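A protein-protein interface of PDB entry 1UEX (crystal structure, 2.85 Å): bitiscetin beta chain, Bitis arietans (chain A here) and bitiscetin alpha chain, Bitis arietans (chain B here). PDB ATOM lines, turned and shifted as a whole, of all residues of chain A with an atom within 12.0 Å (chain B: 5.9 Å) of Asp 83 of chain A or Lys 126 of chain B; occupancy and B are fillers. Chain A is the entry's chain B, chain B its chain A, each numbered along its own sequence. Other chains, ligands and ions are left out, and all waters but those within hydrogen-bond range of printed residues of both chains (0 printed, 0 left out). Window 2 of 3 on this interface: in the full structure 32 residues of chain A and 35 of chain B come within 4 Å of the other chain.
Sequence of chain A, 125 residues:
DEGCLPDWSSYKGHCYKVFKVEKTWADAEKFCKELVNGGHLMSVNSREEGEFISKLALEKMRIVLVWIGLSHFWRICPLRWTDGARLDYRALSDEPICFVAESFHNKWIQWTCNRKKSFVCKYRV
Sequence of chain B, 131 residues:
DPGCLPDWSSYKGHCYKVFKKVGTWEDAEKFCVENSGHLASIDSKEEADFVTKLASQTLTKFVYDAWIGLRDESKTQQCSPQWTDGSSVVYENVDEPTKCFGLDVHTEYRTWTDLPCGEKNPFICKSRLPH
Arg 80 of chain A touches Gly 69 of chain B. Trp 81 of chain A touches Ala 40 of chain B. Trp 81 of chain A touches Ser 41 of chain B. CH2 of Trp 81 of chain A touches N of Ile 42 of chain B, 3.4 Å away. O of Gly 69 of chain B touches CA of Trp 81 of chain A, 2.9 Å away. N of Leu 39 of chain B touches OG1 of Thr 82 of chain A, 3.7 Å away. Asp 83 of chain A touches His 38 of chain B. Asp 43 of chain B touches Ala 85 of chain A (OD1 to CB, 3.5 Å). Tyr 89 of chain A touches Ile 42 of chain B. O of Asp 43 of chain B touches CB of Tyr 89 of chain A (3.1 Å).
The side-chain carboxylate (OE1) of Glu 29 of chain B is in hydrogen-bond range of the backbone NH (N) of Leu 39 of chain B, 2.7 Å away. The backbone NH (N) of Gly 69 of chain B is in hydrogen-bond range of the backbone carbonyl oxygen (O) of Ala 40 of chain B, at 2.7 Å. The backbone NH (N) of Ala 40 of chain B is in hydrogen-bond range of the backbone carbonyl oxygen (O) of Ile 124 of chain B, 2.8 Å away. N of Asp 43 of chain B sits at hydrogen-bond distance from OE2 of Glu 47 of chain B. The side-chain carboxylate (OE1) of Glu 47 of chain B is in salt-bridge range of the side-chain amino group (NZ) of Lys 126 of chain B (3.2 Å). The side-chain sulfur (SG) of Cys 125 of chain B is disulfide-bonded to the side-chain sulfur (SG) of Cys 32 of chain B.
The side-chain hydroxyl (OG1) of Thr 82 of chain A sits at hydrogen-bond distance from the side-chain carboxylate (OE2) of Glu 29 of chain B (2.5 Å). A ring nitrogen (NE2) of His 38 of chain B sits close to the backbone carbonyl oxygen (O) of Thr 82 of chain A, 3.4 Å away. OD1 of Asp 83 of chain A is in hydrogen-bond range of OG of Ser 41 of chain B. O of Gly 69 of chain B sits at hydrogen-bond distance from N of Thr 82 of chain A. OD1 of Asp 83 of chain A lies within salt-bridge range of NZ of Lys 126 of chain B, 3.5 Å away.
Hydrophobic or aromatic side chains of chain A within 4 Å of the printed part of chain B: Trp 81, Ala 85 and Tyr 89. Printed residues of chain B that touch a printed residue of chain A: Glu 29, His 38, Leu 39, Ala 40, Ser 41, Ile 42, Asp 43, Gly 69 and Lys 126. Hydrophobic or aromatic side chains of chain B within 4 Å of the printed part of chain A: His 38 and Ile 42. Among the printed residues, 15 pairs touch across the chains. Among the printed residues, Asp or Glu carboxylates within 4 Å of a Lys or Arg side-chain nitrogen of the other chain: Asp 83 of chain A with Lys 126 of chain B (3.5 Å).
Of chain B, only His 38 (3.3 Å), Ser 41 (2.4 Å) and Lys 126 (3.5 Å) come within 4 Å of Asp 83 of chain A. Lys 126 of chain B touches just one residue of chain A: Asp 83. No residue of chain A comes within 4 Å of Cys 15 of chain B. No residue of chain A comes within 4 Å of Lys 17 of chain B. No residue of chain A comes within 4 Å of Cys 32 of chain B. No residue of chain A comes within 4 Å of Gly 37 of chain B. His 38 of chain B touches two residues of chain A. Ala 40 of chain B touches just one residue of chain A: Trp 81 (3.6 Å). Ser 41 of chain B touches two residues of chain A. Of the printed residues of chain A, Gly 69 of chain B touches Arg 80, Trp 81 and Thr 82. No residue of chain A comes within 4 Å of Cys 125 of chain B. Printed residues of chain A within 4 Å of Leu 39 of chain B: Thr 82 (3.7 Å). Printed residues of chain B within 4 Å of Tyr 89 of chain A: Ile 42 (3.5 Å) and Asp 43 (3.1 Å). Asp 88 of chain A touches none of the printed residues of chain B. Trp 8 of chain B touches none of the printed residues of chain A.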
ATOM      1  N   LEU A  79      -2.576   9.529 -21.359  1.00  0.00           N
ATOM      2  CA  LEU A  79      -1.881   8.255 -21.416  1.00  0.00           C
ATOM      3  C   LEU A  79      -0.412   8.453 -21.057  1.00  0.00           C
ATOM      4  O   LEU A  79       0.280   9.267 -21.671  1.00  0.00           O
ATOM      5  CB  LEU A  79      -2.008   7.652 -22.819  1.00  0.00           C
ATOM      6  CG  LEU A  79      -3.423   7.647 -23.415  1.00  0.00           C
ATOM      7  CD1 LEU A  79      -3.416   6.972 -24.779  1.00  0.00           C
ATOM      8  CD2 LEU A  79      -4.373   6.927 -22.478  1.00  0.00           C
ATOM      9  N   ARG A  80       0.052   7.711 -20.055  1.00  0.00           N
ATOM     10  CA  ARG A  80       1.435   7.793 -19.597  1.00  0.00           C
ATOM     11  C   ARG A  80       2.037   6.398 -19.417  1.00  0.00           C
ATOM     12  O   ARG A  80       1.323   5.429 -19.156  1.00  0.00           O
ATOM     13  CB  ARG A  80       1.509   8.551 -18.262  1.00  0.00           C
ATOM     14  N   TRP A  81       3.352   6.296 -19.569  1.00  0.00           N
ATOM     15  CA  TRP A  81       4.029   5.019 -19.388  1.00  0.00           C
ATOM     16  C   TRP A  81       4.447   4.898 -17.930  1.00  0.00           C
ATOM     17  O   TRP A  81       4.258   5.830 -17.142  1.00  0.00           O
ATOM     18  CB  TRP A  81       5.274   4.917 -20.271  1.00  0.00           C
ATOM     19  CG  TRP A  81       5.011   4.928 -21.745  1.00  0.00           C
ATOM     20  CD1 TRP A  81       5.120   5.990 -22.587  1.00  0.00           C
ATOM     21  CD2 TRP A  81       4.647   3.804 -22.559  1.00  0.00           C
ATOM     22  NE1 TRP A  81       4.856   5.598 -23.879  1.00  0.00           N
ATOM     23  CE2 TRP A  81       4.562   4.260 -23.888  1.00  0.00           C
ATOM     24  CE3 TRP A  81       4.386   2.453 -22.290  1.00  0.00           C
ATOM     25  CZ2 TRP A  81       4.232   3.419 -24.948  1.00  0.00           C
ATOM     26  CZ3 TRP A  81       4.055   1.613 -23.348  1.00  0.00           C
ATOM     27  CH2 TRP A  81       3.981   2.102 -24.659  1.00  0.00           C
ATOM     28  N   THR A  82       5.018   3.754 -17.566  1.00  0.00           N
ATOM     29  CA  THR A  82       5.456   3.548 -16.192  1.00  0.00           C
ATOM     30  C   THR A  82       6.968   3.654 -16.069  1.00  0.00           C
ATOM     31  O   THR A  82       7.494   3.821 -14.967  1.00  0.00           O
ATOM     32  CB  THR A  82       5.002   2.177 -15.638  1.00  0.00           C
ATOM     33  OG1 THR A  82       5.619   1.122 -16.383  1.00  0.00           O
ATOM     34  CG2 THR A  82       3.497   2.045 -15.719  1.00  0.00           C
ATOM     35  N   ASP A  83       7.671   3.556 -17.195  1.00  0.00           N
ATOM     36  CA  ASP A  83       9.120   3.666 -17.150  1.00  0.00           C
ATOM     37  C   ASP A  83       9.542   5.123 -17.333  1.00  0.00           C
ATOM     38  O   ASP A  83      10.717   5.457 -17.179  1.00  0.00           O
ATOM     39  CB  ASP A  83       9.781   2.777 -18.210  1.00  0.00           C
ATOM     40  CG  ASP A  83       9.635   3.322 -19.611  1.00  0.00           C
ATOM     41  OD1 ASP A  83      10.340   2.818 -20.512  1.00  0.00           O
ATOM     42  OD2 ASP A  83       8.820   4.245 -19.814  1.00  0.00           O
ATOM     43  N   GLY A  84       8.583   5.984 -17.667  1.00  0.00           N
ATOM     44  CA  GLY A  84       8.895   7.392 -17.822  1.00  0.00           C
ATOM     45  C   GLY A  84       8.762   8.014 -19.197  1.00  0.00           C
ATOM     46  O   GLY A  84       8.445   9.199 -19.302  1.00  0.00           O
ATOM     47  N   ALA A  85       9.010   7.240 -20.249  1.00  0.00           N
ATOM     48  CA  ALA A  85       8.916   7.756 -21.614  1.00  0.00           C
ATOM     49  C   ALA A  85       7.612   8.518 -21.849  1.00  0.00           C
ATOM     50  O   ALA A  85       6.641   8.354 -21.107  1.00  0.00           O
ATOM     51  CB  ALA A  85       9.044   6.609 -22.620  1.00  0.00           C
ATOM     52  N   ARG A  86       7.604   9.356 -22.884  1.00  0.00           N
ATOM     53  CA  ARG A  86       6.432  10.155 -23.238  1.00  0.00           C
ATOM     54  C   ARG A  86       5.808   9.654 -24.544  1.00  0.00           C
ATOM     55  O   ARG A  86       6.413   9.733 -25.615  1.00  0.00           O
ATOM     56  CB  ARG A  86       6.820  11.636 -23.362  1.00  0.00           C
ATOM     57  CG  ARG A  86       7.204  12.287 -22.032  1.00  0.00           C
ATOM     58  CD  ARG A  86       7.731  13.715 -22.199  1.00  0.00           C
ATOM     59  NE  ARG A  86       8.996  13.762 -22.931  1.00  0.00           N
ATOM     60  CZ  ARG A  86       9.684  14.874 -23.175  1.00  0.00           C
ATOM     61  NH1 ARG A  86       9.231  16.046 -22.746  1.00  0.00           N
ATOM     62  NH2 ARG A  86      10.822  14.818 -23.856  1.00  0.00           N
ATOM     63  N   LEU A  87       4.586   9.137 -24.436  1.00  0.00           N
ATOM     64  CA  LEU A  87       3.848   8.587 -25.567  1.00  0.00           C
ATOM     65  C   LEU A  87       3.680   9.530 -26.752  1.00  0.00           C
ATOM     66  O   LEU A  87       2.875  10.458 -26.716  1.00  0.00           O
ATOM     67  CB  LEU A  87       2.469   8.118 -25.097  1.00  0.00           C
ATOM     68  CG  LEU A  87       1.537   7.536 -26.161  1.00  0.00           C
ATOM     69  CD1 LEU A  87       2.147   6.272 -26.745  1.00  0.00           C
ATOM     70  CD2 LEU A  87       0.185   7.236 -25.539  1.00  0.00           C
ATOM     71  N   ASP A  88       4.445   9.278 -27.806  1.00  0.00           N
ATOM     72  CA  ASP A  88       4.370  10.074 -29.023  1.00  0.00           C
ATOM     73  C   ASP A  88       4.052   9.091 -30.143  1.00  0.00           C
ATOM     74  O   ASP A  88       3.327   9.408 -31.088  1.00  0.00           O
ATOM     75  CB  ASP A  88       5.704  10.776 -29.289  1.00  0.00           C
ATOM     76  CG  ASP A  88       6.058  11.795 -28.214  1.00  0.00           C
ATOM     77  OD1 ASP A  88       5.277  12.751 -28.013  1.00  0.00           O
ATOM     78  OD2 ASP A  88       7.117  11.642 -27.569  1.00  0.00           O
ATOM     79  N   TYR A  89       4.606   7.889 -30.010  1.00  0.00           N
ATOM     80  CA  TYR A  89       4.396   6.805 -30.965  1.00  0.00           C
ATOM     81  C   TYR A  89       3.003   6.245 -30.696  1.00  0.00           C
ATOM     82  O   TYR A  89       2.840   5.347 -29.871  1.00  0.00           O
ATOM     83  CB  TYR A  89       5.456   5.714 -30.748  1.00  0.00           C
ATOM     84  CG  TYR A  89       5.249   4.449 -31.557  1.00  0.00           C
ATOM     85  CD1 TYR A  89       5.438   4.436 -32.940  1.00  0.00           C
ATOM     86  CD2 TYR A  89       4.862   3.262 -30.936  1.00  0.00           C
ATOM     87  CE1 TYR A  89       5.248   3.272 -33.685  1.00  0.00           C
ATOM     88  CE2 TYR A  89       4.667   2.093 -31.669  1.00  0.00           C
ATOM     89  CZ  TYR A  89       4.862   2.104 -33.042  1.00  0.00           C
ATOM     90  OH  TYR A  89       4.668   0.949 -33.768  1.00  0.00           O
ATOM     91  N   TRP B   8      16.146 -13.693 -20.529  1.00  0.00           N
ATOM     92  CA  TRP B   8      15.761 -12.410 -21.116  1.00  0.00           C
ATOM     93  C   TRP B   8      16.410 -12.177 -22.479  1.00  0.00           C
ATOM     94  O   TRP B   8      17.244 -12.968 -22.918  1.00  0.00           O
ATOM     95  CB  TRP B   8      16.132 -11.267 -20.167  1.00  0.00           C
ATOM     96  CG  TRP B   8      15.325 -11.246 -18.902  1.00  0.00           C
ATOM     97  CD1 TRP B   8      15.181 -12.261 -18.006  1.00  0.00           C
ATOM     98  CD2 TRP B   8      14.554 -10.152 -18.394  1.00  0.00           C
ATOM     99  NE1 TRP B   8      14.371 -11.869 -16.969  1.00  0.00           N
ATOM    100  CE2 TRP B   8      13.974 -10.575 -17.182  1.00  0.00           C
ATOM    101  CE3 TRP B   8      14.304  -8.850 -18.845  1.00  0.00           C
ATOM    102  CZ2 TRP B   8      13.151  -9.748 -16.415  1.00  0.00           C
ATOM    103  CZ3 TRP B   8      13.485  -8.025 -18.081  1.00  0.00           C
ATOM    104  CH2 TRP B   8      12.922  -8.479 -16.877  1.00  0.00           C
ATOM    105  N   LYS B  12      19.155  -2.575 -27.699  1.00  0.00           N
ATOM    106  CA  LYS B  12      19.273  -1.131 -27.531  1.00  0.00           C
ATOM    107  C   LYS B  12      19.445  -0.669 -26.079  1.00  0.00           C
ATOM    108  O   LYS B  12      18.809   0.291 -25.644  1.00  0.00           O
ATOM    109  CB  LYS B  12      18.044  -0.455 -28.147  1.00  0.00           C
ATOM    110  CG  LYS B  12      18.051   1.069 -28.124  1.00  0.00           C
ATOM    111  CD  LYS B  12      16.701   1.628 -28.561  1.00  0.00           C
ATOM    112  CE  LYS B  12      15.570   1.142 -27.653  1.00  0.00           C
ATOM    113  NZ  LYS B  12      14.229   1.579 -28.140  1.00  0.00           N
ATOM    114  N   HIS B  14      18.484  -2.121 -23.450  1.00  0.00           N
ATOM    115  CA  HIS B  14      17.286  -2.486 -22.697  1.00  0.00           C
ATOM    116  C   HIS B  14      17.136  -4.002 -22.725  1.00  0.00           C
ATOM    117  O   HIS B  14      17.524  -4.650 -23.696  1.00  0.00           O
ATOM    118  CB  HIS B  14      16.040  -1.839 -23.309  1.00  0.00           C
ATOM    119  CG  HIS B  14      15.969  -0.355 -23.114  1.00  0.00           C
ATOM    120  ND1 HIS B  14      15.923   0.228 -21.872  1.00  0.00           N
ATOM    121  CD2 HIS B  14      15.930   0.658 -24.015  1.00  0.00           C
ATOM    122  CE1 HIS B  14      15.856   1.546 -22.008  1.00  0.00           C
ATOM    123  NE2 HIS B  14      15.859   1.828 -23.295  1.00  0.00           N
ATOM    124  N   CYS B  15      16.582  -4.564 -21.659  1.00  0.00           N
ATOM    125  CA  CYS B  15      16.390  -6.005 -21.582  1.00  0.00           C
ATOM    126  C   CYS B  15      14.915  -6.336 -21.381  1.00  0.00           C
ATOM    127  O   CYS B  15      14.280  -5.826 -20.454  1.00  0.00           O
ATOM    128  CB  CYS B  15      17.222  -6.582 -20.430  1.00  0.00           C
ATOM    129  SG  CYS B  15      19.030  -6.449 -20.646  1.00  0.00           S
ATOM    130  N   TYR B  16      14.373  -7.186 -22.253  1.00  0.00           N
ATOM    131  CA  TYR B  16      12.966  -7.569 -22.170  1.00  0.00           C
ATOM    132  C   TYR B  16      12.791  -9.065 -21.938  1.00  0.00           C
ATOM    133  O   TYR B  16      13.739  -9.843 -22.042  1.00  0.00           O
ATOM    134  CB  TYR B  16      12.216  -7.210 -23.460  1.00  0.00           C
ATOM    135  CG  TYR B  16      12.625  -5.914 -24.125  1.00  0.00           C
ATOM    136  CD1 TYR B  16      13.834  -5.813 -24.815  1.00  0.00           C
ATOM    137  CD2 TYR B  16      11.792  -4.800 -24.092  1.00  0.00           C
ATOM    138  CE1 TYR B  16      14.198  -4.636 -25.462  1.00  0.00           C
ATOM    139  CE2 TYR B  16      12.146  -3.615 -24.735  1.00  0.00           C
ATOM    140  CZ  TYR B  16      13.349  -3.540 -25.418  1.00  0.00           C
ATOM    141  OH  TYR B  16      13.696  -2.376 -26.065  1.00  0.00           O
ATOM    142  N   LYS B  17      11.560  -9.454 -21.629  1.00  0.00           N
ATOM    143  CA  LYS B  17      11.212 -10.849 -21.407  1.00  0.00           C
ATOM    144  C   LYS B  17       9.711 -10.976 -21.224  1.00  0.00           C
ATOM    145  O   LYS B  17       9.106 -10.219 -20.464  1.00  0.00           O
ATOM    146  CB  LYS B  17      11.909 -11.408 -20.167  1.00  0.00           C
ATOM    147  N   GLU B  29       3.264  -4.982 -13.098  1.00  0.00           N
ATOM    148  CA  GLU B  29       4.248  -3.920 -12.944  1.00  0.00           C
ATOM    149  C   GLU B  29       5.037  -4.101 -11.660  1.00  0.00           C
ATOM    150  O   GLU B  29       6.260  -3.935 -11.645  1.00  0.00           O
ATOM    151  CB  GLU B  29       3.567  -2.551 -12.930  1.00  0.00           C
ATOM    152  CG  GLU B  29       4.532  -1.399 -12.729  1.00  0.00           C
ATOM    153  CD  GLU B  29       5.496  -1.224 -13.886  1.00  0.00           C
ATOM    154  OE1 GLU B  29       5.905  -2.237 -14.490  1.00  0.00           O
ATOM    155  OE2 GLU B  29       5.855  -0.070 -14.188  1.00  0.00           O
ATOM    156  N   CYS B  32       7.706  -6.326 -12.584  1.00  0.00           N
ATOM    157  CA  CYS B  32       8.720  -5.776 -13.477  1.00  0.00           C
ATOM    158  C   CYS B  32       9.668  -4.929 -12.652  1.00  0.00           C
ATOM    159  O   CYS B  32      10.877  -4.954 -12.859  1.00  0.00           O
ATOM    160  CB  CYS B  32       8.086  -4.905 -14.564  1.00  0.00           C
ATOM    161  SG  CYS B  32       7.195  -5.807 -15.867  1.00  0.00           S
ATOM    162  N   SER B  36      14.050  -4.620 -11.268  1.00  0.00           N
ATOM    163  CA  SER B  36      14.727  -3.378 -11.623  1.00  0.00           C
ATOM    164  C   SER B  36      14.317  -2.852 -13.001  1.00  0.00           C
ATOM    165  O   SER B  36      15.164  -2.589 -13.857  1.00  0.00           O
ATOM    166  CB  SER B  36      16.241  -3.589 -11.566  1.00  0.00           C
ATOM    167  OG  SER B  36      16.640  -3.930 -10.250  1.00  0.00           O
ATOM    168  N   GLY B  37      13.010  -2.694 -13.200  1.00  0.00           N
ATOM    169  CA  GLY B  37      12.492  -2.198 -14.464  1.00  0.00           C
ATOM    170  C   GLY B  37      11.007  -1.890 -14.398  1.00  0.00           C
ATOM    171  O   GLY B  37      10.453  -1.672 -13.318  1.00  0.00           O
ATOM    172  N   HIS B  38      10.362  -1.862 -15.560  1.00  0.00           N
ATOM    173  CA  HIS B  38       8.929  -1.589 -15.648  1.00  0.00           C
ATOM    174  C   HIS B  38       8.316  -2.389 -16.792  1.00  0.00           C
ATOM    175  O   HIS B  38       9.013  -3.132 -17.485  1.00  0.00           O
ATOM    176  CB  HIS B  38       8.668  -0.098 -15.901  1.00  0.00           C
ATOM    177  CG  HIS B  38       9.265   0.811 -14.874  1.00  0.00           C
ATOM    178  ND1 HIS B  38      10.465   1.462 -15.065  1.00  0.00           N
ATOM    179  CD2 HIS B  38       8.829   1.177 -13.645  1.00  0.00           C
ATOM    180  CE1 HIS B  38      10.742   2.190 -13.997  1.00  0.00           C
ATOM    181  NE2 HIS B  38       9.767   2.034 -13.121  1.00  0.00           N
ATOM    182  N   LEU B  39       7.007  -2.250 -16.974  1.00  0.00           N
ATOM    183  CA  LEU B  39       6.350  -2.938 -18.067  1.00  0.00           C
ATOM    184  C   LEU B  39       6.935  -2.297 -19.318  1.00  0.00           C
ATOM    185  O   LEU B  39       7.206  -1.096 -19.332  1.00  0.00           O
ATOM    186  CB  LEU B  39       4.830  -2.735 -18.007  1.00  0.00           C
ATOM    187  CG  LEU B  39       4.053  -3.617 -17.021  1.00  0.00           C
ATOM    188  CD1 LEU B  39       2.616  -3.143 -16.892  1.00  0.00           C
ATOM    189  CD2 LEU B  39       4.098  -5.055 -17.500  1.00  0.00           C
ATOM    190  N   ALA B  40       7.152  -3.099 -20.353  1.00  0.00           N
ATOM    191  CA  ALA B  40       7.729  -2.604 -21.594  1.00  0.00           C
ATOM    192  C   ALA B  40       7.085  -1.312 -22.068  1.00  0.00           C
ATOM    193  O   ALA B  40       5.886  -1.096 -21.886  1.00  0.00           O
ATOM    194  CB  ALA B  40       7.619  -3.669 -22.679  1.00  0.00           C
ATOM    195  N   SER B  41       7.900  -0.447 -22.667  1.00  0.00           N
ATOM    196  CA  SER B  41       7.427   0.823 -23.203  1.00  0.00           C
ATOM    197  C   SER B  41       7.976   0.922 -24.620  1.00  0.00           C
ATOM    198  O   SER B  41       9.156   0.665 -24.858  1.00  0.00           O
ATOM    199  CB  SER B  41       7.938   1.996 -22.369  1.00  0.00           C
ATOM    200  OG  SER B  41       9.301   2.253 -22.649  1.00  0.00           O
ATOM    201  N   ILE B  42       7.115   1.295 -25.559  1.00  0.00           N
ATOM    202  CA  ILE B  42       7.507   1.407 -26.953  1.00  0.00           C
ATOM    203  C   ILE B  42       7.715   2.860 -27.369  1.00  0.00           C
ATOM    204  O   ILE B  42       6.884   3.724 -27.086  1.00  0.00           O
ATOM    205  CB  ILE B  42       6.438   0.758 -27.846  1.00  0.00           C
ATOM    206  CG1 ILE B  42       6.229  -0.694 -27.402  1.00  0.00           C
ATOM    207  CG2 ILE B  42       6.855   0.835 -29.307  1.00  0.00           C
ATOM    208  CD1 ILE B  42       5.062  -1.387 -28.056  1.00  0.00           C
ATOM    209  N   ASP B  43       8.833   3.118 -28.038  1.00  0.00           N
ATOM    210  CA  ASP B  43       9.170   4.463 -28.499  1.00  0.00           C
ATOM    211  C   ASP B  43       9.236   4.483 -30.015  1.00  0.00           C
ATOM    212  O   ASP B  43       8.515   5.228 -30.678  1.00  0.00           O
ATOM    213  CB  ASP B  43      10.528   4.886 -27.935  1.00  0.00           C
ATOM    214  CG  ASP B  43      10.504   5.065 -26.435  1.00  0.00           C
ATOM    215  OD1 ASP B  43      10.047   6.131 -25.976  1.00  0.00           O
ATOM    216  OD2 ASP B  43      10.930   4.136 -25.717  1.00  0.00           O
ATOM    217  N   GLU B  47      11.522  -0.832 -32.035  1.00  0.00           N
ATOM    218  CA  GLU B  47      11.296  -1.465 -30.743  1.00  0.00           C
ATOM    219  C   GLU B  47       9.883  -2.027 -30.639  1.00  0.00           C
ATOM    220  O   GLU B  47       9.605  -2.868 -29.787  1.00  0.00           O
ATOM    221  CB  GLU B  47      11.529  -0.451 -29.621  1.00  0.00           C
ATOM    222  CG  GLU B  47      11.400  -1.020 -28.216  1.00  0.00           C
ATOM    223  CD  GLU B  47      11.511   0.051 -27.149  1.00  0.00           C
ATOM    224  OE1 GLU B  47      11.577  -0.303 -25.956  1.00  0.00           O
ATOM    225  OE2 GLU B  47      11.530   1.249 -27.503  1.00  0.00           O
ATOM    226  N   GLY B  69       3.539  -1.172 -20.595  1.00  0.00           N
ATOM    227  CA  GLY B  69       3.544  -0.118 -19.593  1.00  0.00           C
ATOM    228  C   GLY B  69       2.791   1.162 -19.886  1.00  0.00           C
ATOM    229  O   GLY B  69       3.259   2.244 -19.540  1.00  0.00           O
ATOM    230  N   ILE B 124       5.006  -8.104 -20.270  1.00  0.00           N
ATOM    231  CA  ILE B 124       6.351  -7.882 -20.777  1.00  0.00           C
ATOM    232  C   ILE B 124       7.084  -6.864 -19.904  1.00  0.00           C
ATOM    233  O   ILE B 124       6.594  -5.753 -19.688  1.00  0.00           O
ATOM    234  CB  ILE B 124       6.309  -7.343 -22.219  1.00  0.00           C
ATOM    235  CG1 ILE B 124       5.314  -8.153 -23.050  1.00  0.00           C
ATOM    236  CG2 ILE B 124       7.690  -7.421 -22.841  1.00  0.00           C
ATOM    237  CD1 ILE B 124       5.052  -7.562 -24.420  1.00  0.00           C
ATOM    238  N   CYS B 125       8.255  -7.248 -19.404  1.00  0.00           N
ATOM    239  CA  CYS B 125       9.059  -6.358 -18.572  1.00  0.00           C
ATOM    240  C   CYS B 125      10.258  -5.822 -19.354  1.00  0.00           C
ATOM    241  O   CYS B 125      10.726  -6.454 -20.301  1.00  0.00           O
ATOM    242  CB  CYS B 125       9.547  -7.087 -17.317  1.00  0.00           C
ATOM    243  SG  CYS B 125       8.256  -7.524 -16.104  1.00  0.00           S
ATOM    244  N   LYS B 126      10.747  -4.655 -18.943  1.00  0.00           N
ATOM    245  CA  LYS B 126      11.879  -4.002 -19.594  1.00  0.00           C
ATOM    246  C   LYS B 126      12.788  -3.353 -18.551  1.00  0.00           C
ATOM    247  O   LYS B 126      12.303  -2.694 -17.629  1.00  0.00           O
ATOM    248  CB  LYS B 126      11.357  -2.940 -20.565  1.00  0.00           C
ATOM    249  CG  LYS B 126      12.404  -2.006 -21.154  1.00  0.00           C
ATOM    250  CD  LYS B 126      11.728  -0.925 -21.989  1.00  0.00           C
ATOM    251  CE  LYS B 126      12.695   0.145 -22.449  1.00  0.00           C
ATOM    252  NZ  LYS B 126      11.984   1.228 -23.184  1.00  0.00           N
ATOM    253  N   SER B 127      14.100  -3.538 -18.696  1.00  0.00           N
ATOM    254  CA  SER B 127      15.071  -2.965 -17.756  1.00  0.00           C
ATOM    255  C   SER B 127      16.222  -2.241 -18.465  1.00  0.00           C
ATOM    256  O   SER B 127      16.186  -2.156 -19.712  1.00  0.00           O
ATOM    257  CB  SER B 127      15.637  -4.062 -16.843  1.00  0.00           C
ATOM    258  OG  SER B 127      14.618  -4.641 -16.041  1.00  0.00           O
